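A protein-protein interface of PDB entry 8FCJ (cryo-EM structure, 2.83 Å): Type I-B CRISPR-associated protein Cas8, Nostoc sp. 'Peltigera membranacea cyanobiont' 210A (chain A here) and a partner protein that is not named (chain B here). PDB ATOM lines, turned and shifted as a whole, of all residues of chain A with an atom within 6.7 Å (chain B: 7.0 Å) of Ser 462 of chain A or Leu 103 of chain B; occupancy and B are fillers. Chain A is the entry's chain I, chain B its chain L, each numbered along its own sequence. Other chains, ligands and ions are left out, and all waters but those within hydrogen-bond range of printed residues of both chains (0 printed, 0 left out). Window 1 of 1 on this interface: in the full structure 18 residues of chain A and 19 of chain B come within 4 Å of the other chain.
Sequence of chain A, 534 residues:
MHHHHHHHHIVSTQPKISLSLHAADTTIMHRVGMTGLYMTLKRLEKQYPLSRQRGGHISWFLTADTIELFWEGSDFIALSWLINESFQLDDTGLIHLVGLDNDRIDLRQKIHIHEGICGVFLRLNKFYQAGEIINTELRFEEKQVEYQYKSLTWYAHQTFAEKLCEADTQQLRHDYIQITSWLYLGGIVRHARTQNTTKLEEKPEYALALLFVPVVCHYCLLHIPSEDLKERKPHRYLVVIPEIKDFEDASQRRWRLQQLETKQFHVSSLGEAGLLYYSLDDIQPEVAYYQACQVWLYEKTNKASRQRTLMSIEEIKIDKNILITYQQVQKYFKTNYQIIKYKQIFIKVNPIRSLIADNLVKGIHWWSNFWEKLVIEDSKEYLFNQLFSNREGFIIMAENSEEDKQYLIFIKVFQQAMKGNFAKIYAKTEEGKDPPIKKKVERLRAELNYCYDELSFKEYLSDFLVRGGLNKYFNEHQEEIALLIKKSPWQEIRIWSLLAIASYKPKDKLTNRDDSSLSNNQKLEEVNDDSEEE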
ATOM      1  N   PHE A 457       8.315   0.774   8.981  1.00  0.00           N
ATOM      2  CA  PHE A 457       7.145   1.621   9.170  1.00  0.00           C
ATOM      3  C   PHE A 457       5.904   0.994   8.562  1.00  0.00           C
ATOM      4  O   PHE A 457       4.827   1.026   9.167  1.00  0.00           O
ATOM      5  CB  PHE A 457       7.367   3.004   8.568  1.00  0.00           C
ATOM      6  CG  PHE A 457       6.125   3.841   8.543  1.00  0.00           C
ATOM      7  CD1 PHE A 457       5.666   4.454   9.695  1.00  0.00           C
ATOM      8  CD2 PHE A 457       5.396   3.990   7.379  1.00  0.00           C
ATOM      9  CE1 PHE A 457       4.518   5.214   9.681  1.00  0.00           C
ATOM     10  CE2 PHE A 457       4.246   4.746   7.361  1.00  0.00           C
ATOM     11  CZ  PHE A 457       3.807   5.360   8.513  1.00  0.00           C
ATOM     12  N   LYS A 458       6.022   0.441   7.355  1.00  0.00           N
ATOM     13  CA  LYS A 458       4.855  -0.162   6.723  1.00  0.00           C
ATOM     14  C   LYS A 458       4.406  -1.404   7.478  1.00  0.00           C
ATOM     15  O   LYS A 458       3.203  -1.647   7.613  1.00  0.00           O
ATOM     16  CB  LYS A 458       5.154  -0.476   5.259  1.00  0.00           C
ATOM     17  CG  LYS A 458       5.336   0.774   4.418  1.00  0.00           C
ATOM     18  CD  LYS A 458       5.223   0.493   2.936  1.00  0.00           C
ATOM     19  CE  LYS A 458       5.444   1.765   2.135  1.00  0.00           C
ATOM     20  NZ  LYS A 458       5.378   1.521   0.670  1.00  0.00           N
ATOM     21  N   GLU A 459       5.351  -2.186   8.003  1.00  0.00           N
ATOM     22  CA  GLU A 459       4.988  -3.333   8.827  1.00  0.00           C
ATOM     23  C   GLU A 459       4.222  -2.893  10.066  1.00  0.00           C
ATOM     24  O   GLU A 459       3.172  -3.460  10.397  1.00  0.00           O
ATOM     25  CB  GLU A 459       6.244  -4.108   9.221  1.00  0.00           C
ATOM     26  CG  GLU A 459       6.004  -5.574   9.523  1.00  0.00           C
ATOM     27  CD  GLU A 459       7.185  -6.442   9.143  1.00  0.00           C
ATOM     28  OE1 GLU A 459       8.308  -5.906   9.048  1.00  0.00           O
ATOM     29  OE2 GLU A 459       6.991  -7.659   8.942  1.00  0.00           O
ATOM     30  N   TYR A 460       4.730  -1.873  10.764  1.00  0.00           N
ATOM     31  CA  TYR A 460       4.052  -1.404  11.968  1.00  0.00           C
ATOM     32  C   TYR A 460       2.676  -0.841  11.647  1.00  0.00           C
ATOM     33  O   TYR A 460       1.706  -1.110  12.364  1.00  0.00           O
ATOM     34  CB  TYR A 460       4.894  -0.350  12.682  1.00  0.00           C
ATOM     35  CG  TYR A 460       4.163   0.280  13.841  1.00  0.00           C
ATOM     36  CD1 TYR A 460       4.010  -0.402  15.039  1.00  0.00           C
ATOM     37  CD2 TYR A 460       3.606   1.545  13.732  1.00  0.00           C
ATOM     38  CE1 TYR A 460       3.334   0.162  16.098  1.00  0.00           C
ATOM     39  CE2 TYR A 460       2.927   2.117  14.786  1.00  0.00           C
ATOM     40  CZ  TYR A 460       2.796   1.420  15.966  1.00  0.00           C
ATOM     41  OH  TYR A 460       2.120   1.986  17.021  1.00  0.00           O
ATOM     42  N   LEU A 461       2.572  -0.049  10.579  1.00  0.00           N
ATOM     43  CA  LEU A 461       1.290   0.536  10.209  1.00  0.00           C
ATOM     44  C   LEU A 461       0.282  -0.539   9.839  1.00  0.00           C
ATOM     45  O   LEU A 461      -0.890  -0.465  10.227  1.00  0.00           O
ATOM     46  CB  LEU A 461       1.476   1.516   9.052  1.00  0.00           C
ATOM     47  CG  LEU A 461       0.202   1.970   8.345  1.00  0.00           C
ATOM     48  CD1 LEU A 461      -0.637   2.827   9.272  1.00  0.00           C
ATOM     49  CD2 LEU A 461       0.539   2.721   7.072  1.00  0.00           C
ATOM     50  N   SER A 462       0.717  -1.550   9.087  1.00  0.00           N
ATOM     51  CA  SER A 462      -0.179  -2.631   8.705  1.00  0.00           C
ATOM     52  C   SER A 462      -0.643  -3.420   9.923  1.00  0.00           C
ATOM     53  O   SER A 462      -1.830  -3.758  10.037  1.00  0.00           O
ATOM     54  CB  SER A 462       0.523  -3.540   7.704  1.00  0.00           C
ATOM     55  OG  SER A 462      -0.352  -4.544   7.242  1.00  0.00           O
ATOM     56  N   ASP A 463       0.274  -3.718  10.845  1.00  0.00           N
ATOM     57  CA  ASP A 463      -0.112  -4.427  12.059  1.00  0.00           C
ATOM     58  C   ASP A 463      -1.082  -3.599  12.892  1.00  0.00           C
ATOM     59  O   ASP A 463      -2.028  -4.138  13.476  1.00  0.00           O
ATOM     60  CB  ASP A 463       1.128  -4.789  12.872  1.00  0.00           C
ATOM     61  CG  ASP A 463       0.801  -5.609  14.102  1.00  0.00           C
ATOM     62  OD1 ASP A 463       0.480  -5.010  15.149  1.00  0.00           O
ATOM     63  OD2 ASP A 463       0.863  -6.853  14.022  1.00  0.00           O
ATOM     64  N   PHE A 464      -0.859  -2.286  12.959  1.00  0.00           N
ATOM     65  CA  PHE A 464      -1.775  -1.404  13.677  1.00  0.00           C
ATOM     66  C   PHE A 464      -3.158  -1.411  13.038  1.00  0.00           C
ATOM     67  O   PHE A 464      -4.176  -1.478  13.739  1.00  0.00           O
ATOM     68  CB  PHE A 464      -1.198   0.009  13.705  1.00  0.00           C
ATOM     69  CG  PHE A 464      -2.001   0.983  14.510  1.00  0.00           C
ATOM     70  CD1 PHE A 464      -1.885   1.022  15.887  1.00  0.00           C
ATOM     71  CD2 PHE A 464      -2.858   1.871  13.889  1.00  0.00           C
ATOM     72  CE1 PHE A 464      -2.617   1.921  16.629  1.00  0.00           C
ATOM     73  CE2 PHE A 464      -3.593   2.771  14.628  1.00  0.00           C
ATOM     74  CZ  PHE A 464      -3.471   2.796  15.999  1.00  0.00           C
ATOM     75  N   LEU A 465      -3.213  -1.354  11.706  1.00  0.00           N
ATOM     76  CA  LEU A 465      -4.496  -1.393  11.014  1.00  0.00           C
ATOM     77  C   LEU A 465      -5.229  -2.697  11.294  1.00  0.00           C
ATOM     78  O   LEU A 465      -6.446  -2.697  11.516  1.00  0.00           O
ATOM     79  CB  LEU A 465      -4.292  -1.209   9.511  1.00  0.00           C
ATOM     80  CG  LEU A 465      -3.807   0.155   9.020  1.00  0.00           C
ATOM     81  CD1 LEU A 465      -3.659   0.151   7.511  1.00  0.00           C
ATOM     82  CD2 LEU A 465      -4.755   1.250   9.457  1.00  0.00           C
ATOM     83  N   VAL A 466      -4.509  -3.820  11.280  1.00  0.00           N
ATOM     84  CA  VAL A 466      -5.147  -5.101  11.569  1.00  0.00           C
ATOM     85  C   VAL A 466      -5.644  -5.144  13.008  1.00  0.00           C
ATOM     86  O   VAL A 466      -6.764  -5.591  13.278  1.00  0.00           O
ATOM     87  CB  VAL A 466      -4.188  -6.265  11.272  1.00  0.00           C
ATOM     88  CG1 VAL A 466      -4.857  -7.580  11.603  1.00  0.00           C
ATOM     89  CG2 VAL A 466      -3.780  -6.240   9.824  1.00  0.00           C
ATOM     90  N   ARG A 467      -4.821  -4.688  13.955  1.00  0.00           N
ATOM     91  CA  ARG A 467      -5.229  -4.675  15.353  1.00  0.00           C
ATOM     92  C   ARG A 467      -6.400  -3.731  15.594  1.00  0.00           C
ATOM     93  O   ARG A 467      -7.116  -3.889  16.587  1.00  0.00           O
ATOM     94  CB  ARG A 467      -4.038  -4.294  16.238  1.00  0.00           C
ATOM     95  CG  ARG A 467      -4.317  -4.350  17.732  1.00  0.00           C
ATOM     96  CD  ARG A 467      -3.037  -4.331  18.553  1.00  0.00           C
ATOM     97  NE  ARG A 467      -2.139  -3.254  18.158  1.00  0.00           N
ATOM     98  CZ  ARG A 467      -0.990  -3.435  17.520  1.00  0.00           C
ATOM     99  NH1 ARG A 467      -0.566  -4.644  17.192  1.00  0.00           N
ATOM    100  NH2 ARG A 467      -0.248  -2.378  17.207  1.00  0.00           N
ATOM    101  N   PHE A 474     -11.472   1.321   5.072  1.00  0.00           N
ATOM    102  CA  PHE A 474     -10.539   0.535   4.272  1.00  0.00           C
ATOM    103  C   PHE A 474     -11.284  -0.390   3.319  1.00  0.00           C
ATOM    104  O   PHE A 474     -10.906  -0.529   2.150  1.00  0.00           O
ATOM    105  CB  PHE A 474      -9.613  -0.266   5.188  1.00  0.00           C
ATOM    106  CG  PHE A 474      -8.273  -0.584   4.581  1.00  0.00           C
ATOM    107  CD1 PHE A 474      -8.066  -0.495   3.216  1.00  0.00           C
ATOM    108  CD2 PHE A 474      -7.216  -0.971   5.383  1.00  0.00           C
ATOM    109  CE1 PHE A 474      -6.839  -0.790   2.666  1.00  0.00           C
ATOM    110  CE2 PHE A 474      -5.986  -1.265   4.837  1.00  0.00           C
ATOM    111  CZ  PHE A 474      -5.797  -1.174   3.477  1.00  0.00           C
ATOM    112  N   ILE A 481      -6.649   2.683  -1.148  1.00  0.00           N
ATOM    113  CA  ILE A 481      -5.824   2.783   0.050  1.00  0.00           C
ATOM    114  C   ILE A 481      -4.655   1.809  -0.017  1.00  0.00           C
ATOM    115  O   ILE A 481      -3.547   2.119   0.433  1.00  0.00           O
ATOM    116  CB  ILE A 481      -6.681   2.564   1.309  1.00  0.00           C
ATOM    117  CG1 ILE A 481      -7.764   3.637   1.404  1.00  0.00           C
ATOM    118  CG2 ILE A 481      -5.818   2.603   2.555  1.00  0.00           C
ATOM    119  CD1 ILE A 481      -7.227   5.046   1.323  1.00  0.00           C
ATOM    120  N   ALA A 482      -4.879   0.616  -0.574  1.00  0.00           N
ATOM    121  CA  ALA A 482      -3.792  -0.348  -0.705  1.00  0.00           C
ATOM    122  C   ALA A 482      -2.690   0.188  -1.611  1.00  0.00           C
ATOM    123  O   ALA A 482      -1.501   0.113  -1.276  1.00  0.00           O
ATOM    124  CB  ALA A 482      -4.333  -1.674  -1.235  1.00  0.00           C
ATOM    125  N   LEU A 483      -3.071   0.754  -2.759  1.00  0.00           N
ATOM    126  CA  LEU A 483      -2.084   1.346  -3.653  1.00  0.00           C
ATOM    127  C   LEU A 483      -1.389   2.526  -2.993  1.00  0.00           C
ATOM    128  O   LEU A 483      -0.181   2.722  -3.166  1.00  0.00           O
ATOM    129  CB  LEU A 483      -2.751   1.783  -4.957  1.00  0.00           C
ATOM    130  CG  LEU A 483      -2.579   0.840  -6.144  1.00  0.00           C
ATOM    131  CD1 LEU A 483      -1.113   0.723  -6.502  1.00  0.00           C
ATOM    132  CD2 LEU A 483      -3.162  -0.518  -5.828  1.00  0.00           C
ATOM    133  N   ILE A 485      -0.808   3.029   0.242  1.00  0.00           N
ATOM    134  CA  ILE A 485       0.150   2.537   1.224  1.00  0.00           C
ATOM    135  C   ILE A 485       1.365   1.935   0.533  1.00  0.00           C
ATOM    136  O   ILE A 485       2.508   2.173   0.941  1.00  0.00           O
ATOM    137  CB  ILE A 485      -0.524   1.528   2.169  1.00  0.00           C
ATOM    138  CG1 ILE A 485      -1.536   2.239   3.068  1.00  0.00           C
ATOM    139  CG2 ILE A 485       0.513   0.803   3.007  1.00  0.00           C
ATOM    140  CD1 ILE A 485      -2.109   1.363   4.156  1.00  0.00           C
ATOM    141  N   LYS A 486       1.146   1.151  -0.526  1.00  0.00           N
ATOM    142  CA  LYS A 486       2.265   0.485  -1.186  1.00  0.00           C
ATOM    143  C   LYS A 486       3.190   1.480  -1.877  1.00  0.00           C
ATOM    144  O   LYS A 486       4.416   1.325  -1.835  1.00  0.00           O
ATOM    145  CB  LYS A 486       1.742  -0.543  -2.187  1.00  0.00           C
ATOM    146  CG  LYS A 486       2.811  -1.110  -3.104  1.00  0.00           C
ATOM    147  CD  LYS A 486       2.342  -2.386  -3.781  1.00  0.00           C
ATOM    148  CE  LYS A 486       3.456  -3.011  -4.601  1.00  0.00           C
ATOM    149  NZ  LYS A 486       4.785  -2.803  -3.968  1.00  0.00           N
ATOM    150  N   TYR B  11      -0.055  -7.174  -7.217  1.00  0.00           N
ATOM    151  CA  TYR B  11      -0.259  -6.908  -5.797  1.00  0.00           C
ATOM    152  C   TYR B  11      -1.742  -6.930  -5.439  1.00  0.00           C
ATOM    153  O   TYR B  11      -2.142  -7.536  -4.436  1.00  0.00           O
ATOM    154  CB  TYR B  11       0.384  -5.567  -5.448  1.00  0.00           C
ATOM    155  CG  TYR B  11      -0.114  -4.904  -4.190  1.00  0.00           C
ATOM    156  CD1 TYR B  11       0.230  -5.394  -2.941  1.00  0.00           C
ATOM    157  CD2 TYR B  11      -0.903  -3.766  -4.253  1.00  0.00           C
ATOM    158  CE1 TYR B  11      -0.213  -4.781  -1.790  1.00  0.00           C
ATOM    159  CE2 TYR B  11      -1.350  -3.145  -3.108  1.00  0.00           C
ATOM    160  CZ  TYR B  11      -1.002  -3.656  -1.880  1.00  0.00           C
ATOM    161  OH  TYR B  11      -1.447  -3.041  -0.737  1.00  0.00           O
ATOM    162  N   ILE B  15      -3.838  -9.528  -3.061  1.00  0.00           N
ATOM    163  CA  ILE B  15      -4.735  -9.102  -1.989  1.00  0.00           C
ATOM    164  C   ILE B  15      -6.075  -9.815  -2.110  1.00  0.00           C
ATOM    165  O   ILE B  15      -6.626 -10.321  -1.123  1.00  0.00           O
ATOM    166  CB  ILE B  15      -4.907  -7.573  -2.004  1.00  0.00           C
ATOM    167  CG1 ILE B  15      -3.613  -6.889  -1.560  1.00  0.00           C
ATOM    168  CG2 ILE B  15      -6.068  -7.162  -1.116  1.00  0.00           C
ATOM    169  CD1 ILE B  15      -3.815  -5.507  -0.986  1.00  0.00           C
ATOM    170  N   PHE B  18      -5.713 -13.518  -1.104  1.00  0.00           N
ATOM    171  CA  PHE B  18      -5.679 -13.694   0.341  1.00  0.00           C
ATOM    172  C   PHE B  18      -7.054 -13.472   0.954  1.00  0.00           C
ATOM    173  O   PHE B  18      -7.449 -14.187   1.880  1.00  0.00           O
ATOM    174  CB  PHE B  18      -4.652 -12.756   0.970  1.00  0.00           C
ATOM    175  CG  PHE B  18      -4.225 -13.171   2.345  1.00  0.00           C
ATOM    176  CD1 PHE B  18      -4.914 -12.733   3.458  1.00  0.00           C
ATOM    177  CD2 PHE B  18      -3.139 -14.006   2.523  1.00  0.00           C
ATOM    178  CE1 PHE B  18      -4.526 -13.117   4.723  1.00  0.00           C
ATOM    179  CE2 PHE B  18      -2.748 -14.394   3.787  1.00  0.00           C
ATOM    180  CZ  PHE B  18      -3.443 -13.947   4.888  1.00  0.00           C
ATOM    181  N   GLN B  19      -7.798 -12.484   0.453  1.00  0.00           N
ATOM    182  CA  GLN B  19      -9.135 -12.239   0.984  1.00  0.00           C
ATOM    183  C   GLN B  19     -10.059 -13.420   0.721  1.00  0.00           C
ATOM    184  O   GLN B  19     -10.853 -13.802   1.587  1.00  0.00           O
ATOM    185  CB  GLN B  19      -9.707 -10.954   0.388  1.00  0.00           C
ATOM    186  CG  GLN B  19      -9.096  -9.698   0.975  1.00  0.00           C
ATOM    187  CD  GLN B  19      -9.780  -8.439   0.496  1.00  0.00           C
ATOM    188  OE1 GLN B  19      -9.497  -7.345   0.979  1.00  0.00           O
ATOM    189  NE2 GLN B  19     -10.689  -8.586  -0.459  1.00  0.00           N
ATOM    190  N   ARG B  49      -3.995 -12.636  12.710  1.00  0.00           N
ATOM    191  CA  ARG B  49      -2.923 -11.664  12.887  1.00  0.00           C
ATOM    192  C   ARG B  49      -1.808 -12.222  13.760  1.00  0.00           C
ATOM    193  O   ARG B  49      -0.623 -12.046  13.453  1.00  0.00           O
ATOM    194  CB  ARG B  49      -3.472 -10.375  13.492  1.00  0.00           C
ATOM    195  CG  ARG B  49      -2.435  -9.276  13.630  1.00  0.00           C
ATOM    196  CD  ARG B  49      -2.865  -8.233  14.644  1.00  0.00           C
ATOM    197  NE  ARG B  49      -2.731  -8.716  16.012  1.00  0.00           N
ATOM    198  CZ  ARG B  49      -1.654  -8.536  16.765  1.00  0.00           C
ATOM    199  NH1 ARG B  49      -0.596  -7.884  16.312  1.00  0.00           N
ATOM    200  NH2 ARG B  49      -1.640  -9.020  18.003  1.00  0.00           N
ATOM    201  N   ILE B  97       5.398  -9.661   1.663  1.00  0.00           N
ATOM    202  CA  ILE B  97       4.212 -10.495   1.500  1.00  0.00           C
ATOM    203  C   ILE B  97       3.378 -10.483   2.773  1.00  0.00           C
ATOM    204  O   ILE B  97       2.143 -10.480   2.720  1.00  0.00           O
ATOM    205  CB  ILE B  97       4.607 -11.924   1.088  1.00  0.00           C
ATOM    206  CG1 ILE B  97       5.364 -11.907  -0.237  1.00  0.00           C
ATOM    207  CG2 ILE B  97       3.378 -12.794   0.948  1.00  0.00           C
ATOM    208  CD1 ILE B  97       6.448 -12.946  -0.321  1.00  0.00           C
ATOM    209  N   ARG B  98       4.030 -10.471   3.937  1.00  0.00           N
ATOM    210  CA  ARG B  98       3.289 -10.364   5.191  1.00  0.00           C
ATOM    211  C   ARG B  98       2.575  -9.025   5.293  1.00  0.00           C
ATOM    212  O   ARG B  98       1.441  -8.952   5.783  1.00  0.00           O
ATOM    213  CB  ARG B  98       4.225 -10.564   6.380  1.00  0.00           C
ATOM    214  CG  ARG B  98       3.531 -10.438   7.722  1.00  0.00           C
ATOM    215  CD  ARG B  98       4.332 -11.089   8.831  1.00  0.00           C
ATOM    216  NE  ARG B  98       5.407 -10.226   9.302  1.00  0.00           N
ATOM    217  CZ  ARG B  98       6.340 -10.600  10.166  1.00  0.00           C
ATOM    218  NH1 ARG B  98       6.358 -11.819  10.677  1.00  0.00           N
ATOM    219  NH2 ARG B  98       7.277  -9.729  10.525  1.00  0.00           N
ATOM    220  N   ILE B  99       3.224  -7.951   4.843  1.00  0.00           N
ATOM    221  CA  ILE B  99       2.579  -6.641   4.843  1.00  0.00           C
ATOM    222  C   ILE B  99       1.338  -6.660   3.962  1.00  0.00           C
ATOM    223  O   ILE B  99       0.275  -6.157   4.346  1.00  0.00           O
ATOM    224  CB  ILE B  99       3.573  -5.554   4.396  1.00  0.00           C
ATOM    225  CG1 ILE B  99       4.677  -5.380   5.437  1.00  0.00           C
ATOM    226  CG2 ILE B  99       2.853  -4.239   4.160  1.00  0.00           C
ATOM    227  CD1 ILE B  99       5.563  -4.185   5.189  1.00  0.00           C
ATOM    228  N   TRP B 100       1.451  -7.246   2.768  1.00  0.00           N
ATOM    229  CA  TRP B 100       0.299  -7.327   1.874  1.00  0.00           C
ATOM    230  C   TRP B 100      -0.807  -8.187   2.474  1.00  0.00           C
ATOM    231  O   TRP B 100      -1.993  -7.863   2.348  1.00  0.00           O
ATOM    232  CB  TRP B 100       0.717  -7.877   0.512  1.00  0.00           C
ATOM    233  CG  TRP B 100       1.866  -7.162  -0.111  1.00  0.00           C
ATOM    234  CD1 TRP B 100       2.308  -5.907   0.180  1.00  0.00           C
ATOM    235  CD2 TRP B 100       2.723  -7.662  -1.141  1.00  0.00           C
ATOM    236  NE1 TRP B 100       3.391  -5.594  -0.602  1.00  0.00           N
ATOM    237  CE2 TRP B 100       3.665  -6.656  -1.423  1.00  0.00           C
ATOM    238  CE3 TRP B 100       2.786  -8.863  -1.850  1.00  0.00           C
ATOM    239  CZ2 TRP B 100       4.658  -6.815  -2.383  1.00  0.00           C
ATOM    240  CZ3 TRP B 100       3.771  -9.018  -2.801  1.00  0.00           C
ATOM    241  CH2 TRP B 100       4.693  -8.000  -3.060  1.00  0.00           C
ATOM    242  N   SER B 101      -0.438  -9.294   3.121  1.00  0.00           N
ATOM    243  CA  SER B 101      -1.434 -10.159   3.742  1.00  0.00           C
ATOM    244  C   SER B 101      -2.172  -9.437   4.859  1.00  0.00           C
ATOM    245  O   SER B 101      -3.395  -9.560   4.988  1.00  0.00           O
ATOM    246  CB  SER B 101      -0.766 -11.425   4.276  1.00  0.00           C
ATOM    247  OG  SER B 101       0.297 -11.827   3.434  1.00  0.00           O
ATOM    248  N   LEU B 102      -1.448  -8.677   5.679  1.00  0.00           N
ATOM    249  CA  LEU B 102      -2.104  -7.932   6.745  1.00  0.00           C
ATOM    250  C   LEU B 102      -2.969  -6.806   6.192  1.00  0.00           C
ATOM    251  O   LEU B 102      -4.035  -6.518   6.746  1.00  0.00           O
ATOM    252  CB  LEU B 102      -1.063  -7.393   7.723  1.00  0.00           C
ATOM    253  CG  LEU B 102      -0.325  -8.410   8.591  1.00  0.00           C
ATOM    254  CD1 LEU B 102       0.948  -7.800   9.147  1.00  0.00           C
ATOM    255  CD2 LEU B 102      -1.217  -8.902   9.713  1.00  0.00           C
ATOM    256  N   LEU B 103      -2.541  -6.164   5.104  1.00  0.00           N
ATOM    257  CA  LEU B 103      -3.404  -5.184   4.447  1.00  0.00           C
ATOM    258  C   LEU B 103      -4.686  -5.834   3.946  1.00  0.00           C
ATOM    259  O   LEU B 103      -5.776  -5.262   4.077  1.00  0.00           O
ATOM    260  CB  LEU B 103      -2.657  -4.511   3.298  1.00  0.00           C
ATOM    261  CG  LEU B 103      -2.213  -3.064   3.513  1.00  0.00           C
ATOM    262  CD1 LEU B 103      -1.563  -2.891   4.861  1.00  0.00           C
ATOM    263  CD2 LEU B 103      -1.255  -2.642   2.419  1.00  0.00           C
ATOM    264  N   ALA B 104      -4.575  -7.031   3.369  1.00  0.00           N
ATOM    265  CA  ALA B 104      -5.763  -7.756   2.929  1.00  0.00           C
ATOM    266  C   ALA B 104      -6.662  -8.101   4.108  1.00  0.00           C
ATOM    267  O   ALA B 104      -7.892  -8.048   3.998  1.00  0.00           O
ATOM    268  CB  ALA B 104      -5.357  -9.020   2.176  1.00  0.00           C
ATOM    269  N   ILE B 105      -6.064  -8.470   5.242  1.00  0.00           N
ATOM    270  CA  ILE B 105      -6.845  -8.753   6.444  1.00  0.00           C
ATOM    271  C   ILE B 105      -7.614  -7.513   6.874  1.00  0.00           C
ATOM    272  O   ILE B 105      -8.811  -7.571   7.178  1.00  0.00           O
ATOM    273  CB  ILE B 105      -5.929  -9.253   7.574  1.00  0.00           C
ATOM    274  CG1 ILE B 105      -5.511 -10.699   7.344  1.00  0.00           C
ATOM    275  CG2 ILE B 105      -6.639  -9.149   8.909  1.00  0.00           C
ATOM    276  CD1 ILE B 105      -4.438 -11.163   8.288  1.00  0.00           C
ATOM    277  N   ALA B 106      -6.930  -6.369   6.902  1.00  0.00           N
ATOM    278  CA  ALA B 106      -7.560  -5.130   7.349  1.00  0.00           C
ATOM    279  C   ALA B 106      -8.678  -4.702   6.408  1.00  0.00           C
ATOM    280  O   ALA B 106      -9.719  -4.209   6.858  1.00  0.00           O
ATOM    281  CB  ALA B 106      -6.514  -4.025   7.476  1.00  0.00           C
ATOM    282  N   SER B 107      -8.486  -4.881   5.101  1.00  0.00           N
ATOM    283  CA  SER B 107      -9.459  -4.448   4.105  1.00  0.00           C
ATOM    284  C   SER B 107     -10.478  -5.527   3.767  1.00  0.00           C
ATOM    285  O   SER B 107     -11.014  -5.540   2.653  1.00  0.00           O
ATOM    286  CB  SER B 107      -8.739  -3.984   2.839  1.00  0.00           C
ATOM    287  OG  SER B 107      -8.197  -5.085   2.134  1.00  0.00           O
ATOM    288  N   TYR B 108     -10.764  -6.433   4.696  1.00  0.00           N
ATOM    289  CA  TYR B 108     -11.667  -7.545   4.437  1.00  0.00           C
ATOM    290  C   TYR B 108     -13.083  -7.212   4.883  1.00  0.00           C
ATOM    291  O   TYR B 108     -13.294  -6.642   5.958  1.00  0.00           O
ATOM    292  CB  TYR B 108     -11.183  -8.802   5.155  1.00  0.00           C
ATOM    293  CG  TYR B 108     -12.147  -9.962   5.078  1.00  0.00           C
ATOM    294  CD1 TYR B 108     -12.445 -10.565   3.866  1.00  0.00           C
ATOM    295  CD2 TYR B 108     -12.753 -10.459   6.223  1.00  0.00           C
ATOM    296  CE1 TYR B 108     -13.322 -11.626   3.795  1.00  0.00           C
ATOM    297  CE2 TYR B 108     -13.631 -11.519   6.162  1.00  0.00           C
ATOM    298  CZ  TYR B 108     -13.912 -12.099   4.947  1.00  0.00           C
ATOM    299  OH  TYR B 108     -14.788 -13.156   4.887  1.00  0.00           O
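Of the 17 printed residues of chain A, 10 touch a printed residue of chain B.
Printed residues of chain A that touch a printed residue of chain B: Lys 458, Glu 459, Ser 462, Asp 463, Val 466, Arg 467, Phe 474, Ala 482, Ile 485 and Lys 486.
Of the 17 printed residues of chain B, 10 touch a printed residue of chain A.
Hydrophobic or aromatic side chains of chain B within 4 Å of the printed part of chain A: Tyr 11, Ile 15, Ile 99, Leu 102, Leu 103, Ile 105 and Ala 106.
Among the printed residues, pairs that only touch across the chains: Lys 458 of chain A with Ile 99 of chain B, Glu 459 of chain A with Ile 99 of chain B, Ser 462 of chain A with Leu 102 of chain B, Val 466 of chain A with Arg 49 of chain B, Val 466 of chain A with Leu 102 of chain B, Val 466 of chain A with Ile 105 of chain B, Phe 474 of chain A with Ala 106 of chain B, Phe 474 of chain A with Ser 107 of chain B, Ala 482 of chain A with Ile 15 of chain B, Ile 485 of chain A with Leu 103 of chain B and Lys 486 of chain A with Tyr 11 of chain B.
NZ of Lys 458 of chain A sits at hydrogen-bond distance from O of Ile 485 of chain A (3.0 Å).
The side-chain hydroxyl (OG) of Ser 107 of chain B is in hydrogen-bond range of the side-chain amide oxygen (OE1) of Gln 19 of chain B, 2.9 Å away.
The guanidinium group (NH2) of Arg 98 of chain B lies within salt-bridge range of the side-chain carboxylate (OE2) of Glu 459 of chain A (2.6 Å).
The side-chain hydroxyl (OG) of Ser 462 of chain A lies within hydrogen-bond range of the backbone carbonyl oxygen (O) of Ile 99 of chain B.
OG of Ser 462 of chain A lies close to N of Leu 103 of chain B (3.5 Å).
The guanidinium group (NH1) of Arg 49 of chain B lies within salt-bridge range of the side-chain carboxylate (OD2) of Asp 463 of chain A (2.9 Å).
The side-chain hydroxyl of Tyr 11 of chain B is in hydrogen-bond range of the backbone carbonyl oxygen of Ala 482 of chain A, 3.2 Å away.
NH1 of Arg 49 of chain B lies close to NH1 of Arg 467 of chain A (3.4 Å).
Of chain B, only Ile 99 (3.4 Å), Leu 102 (3.0 Å) and Leu 103 (3.1 Å) come within 4 Å of Ser 462 of chain A.
Of the printed residues of chain B, Phe 474 of chain A touches Ala 106 (3.8 Å) and Ser 107 (3.6 Å).
Of the printed residues of chain B, Glu 459 of chain A touches Arg 98 (2.6 Å) and Ile 99 (3.5 Å).
Of the printed residues of chain B, Ile 485 of chain A touches Leu 103 (3.9 Å).
Trp 100 of chain B touches none of the printed residues of chain A.
The nearest residue of chain B that does not touch Ser 462 of chain A is Arg 98 of chain B (5.0 Å).
The nearest printed residue of chain A that does not touch Arg 49 of chain B is Phe 464 of chain A (6.5 Å).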
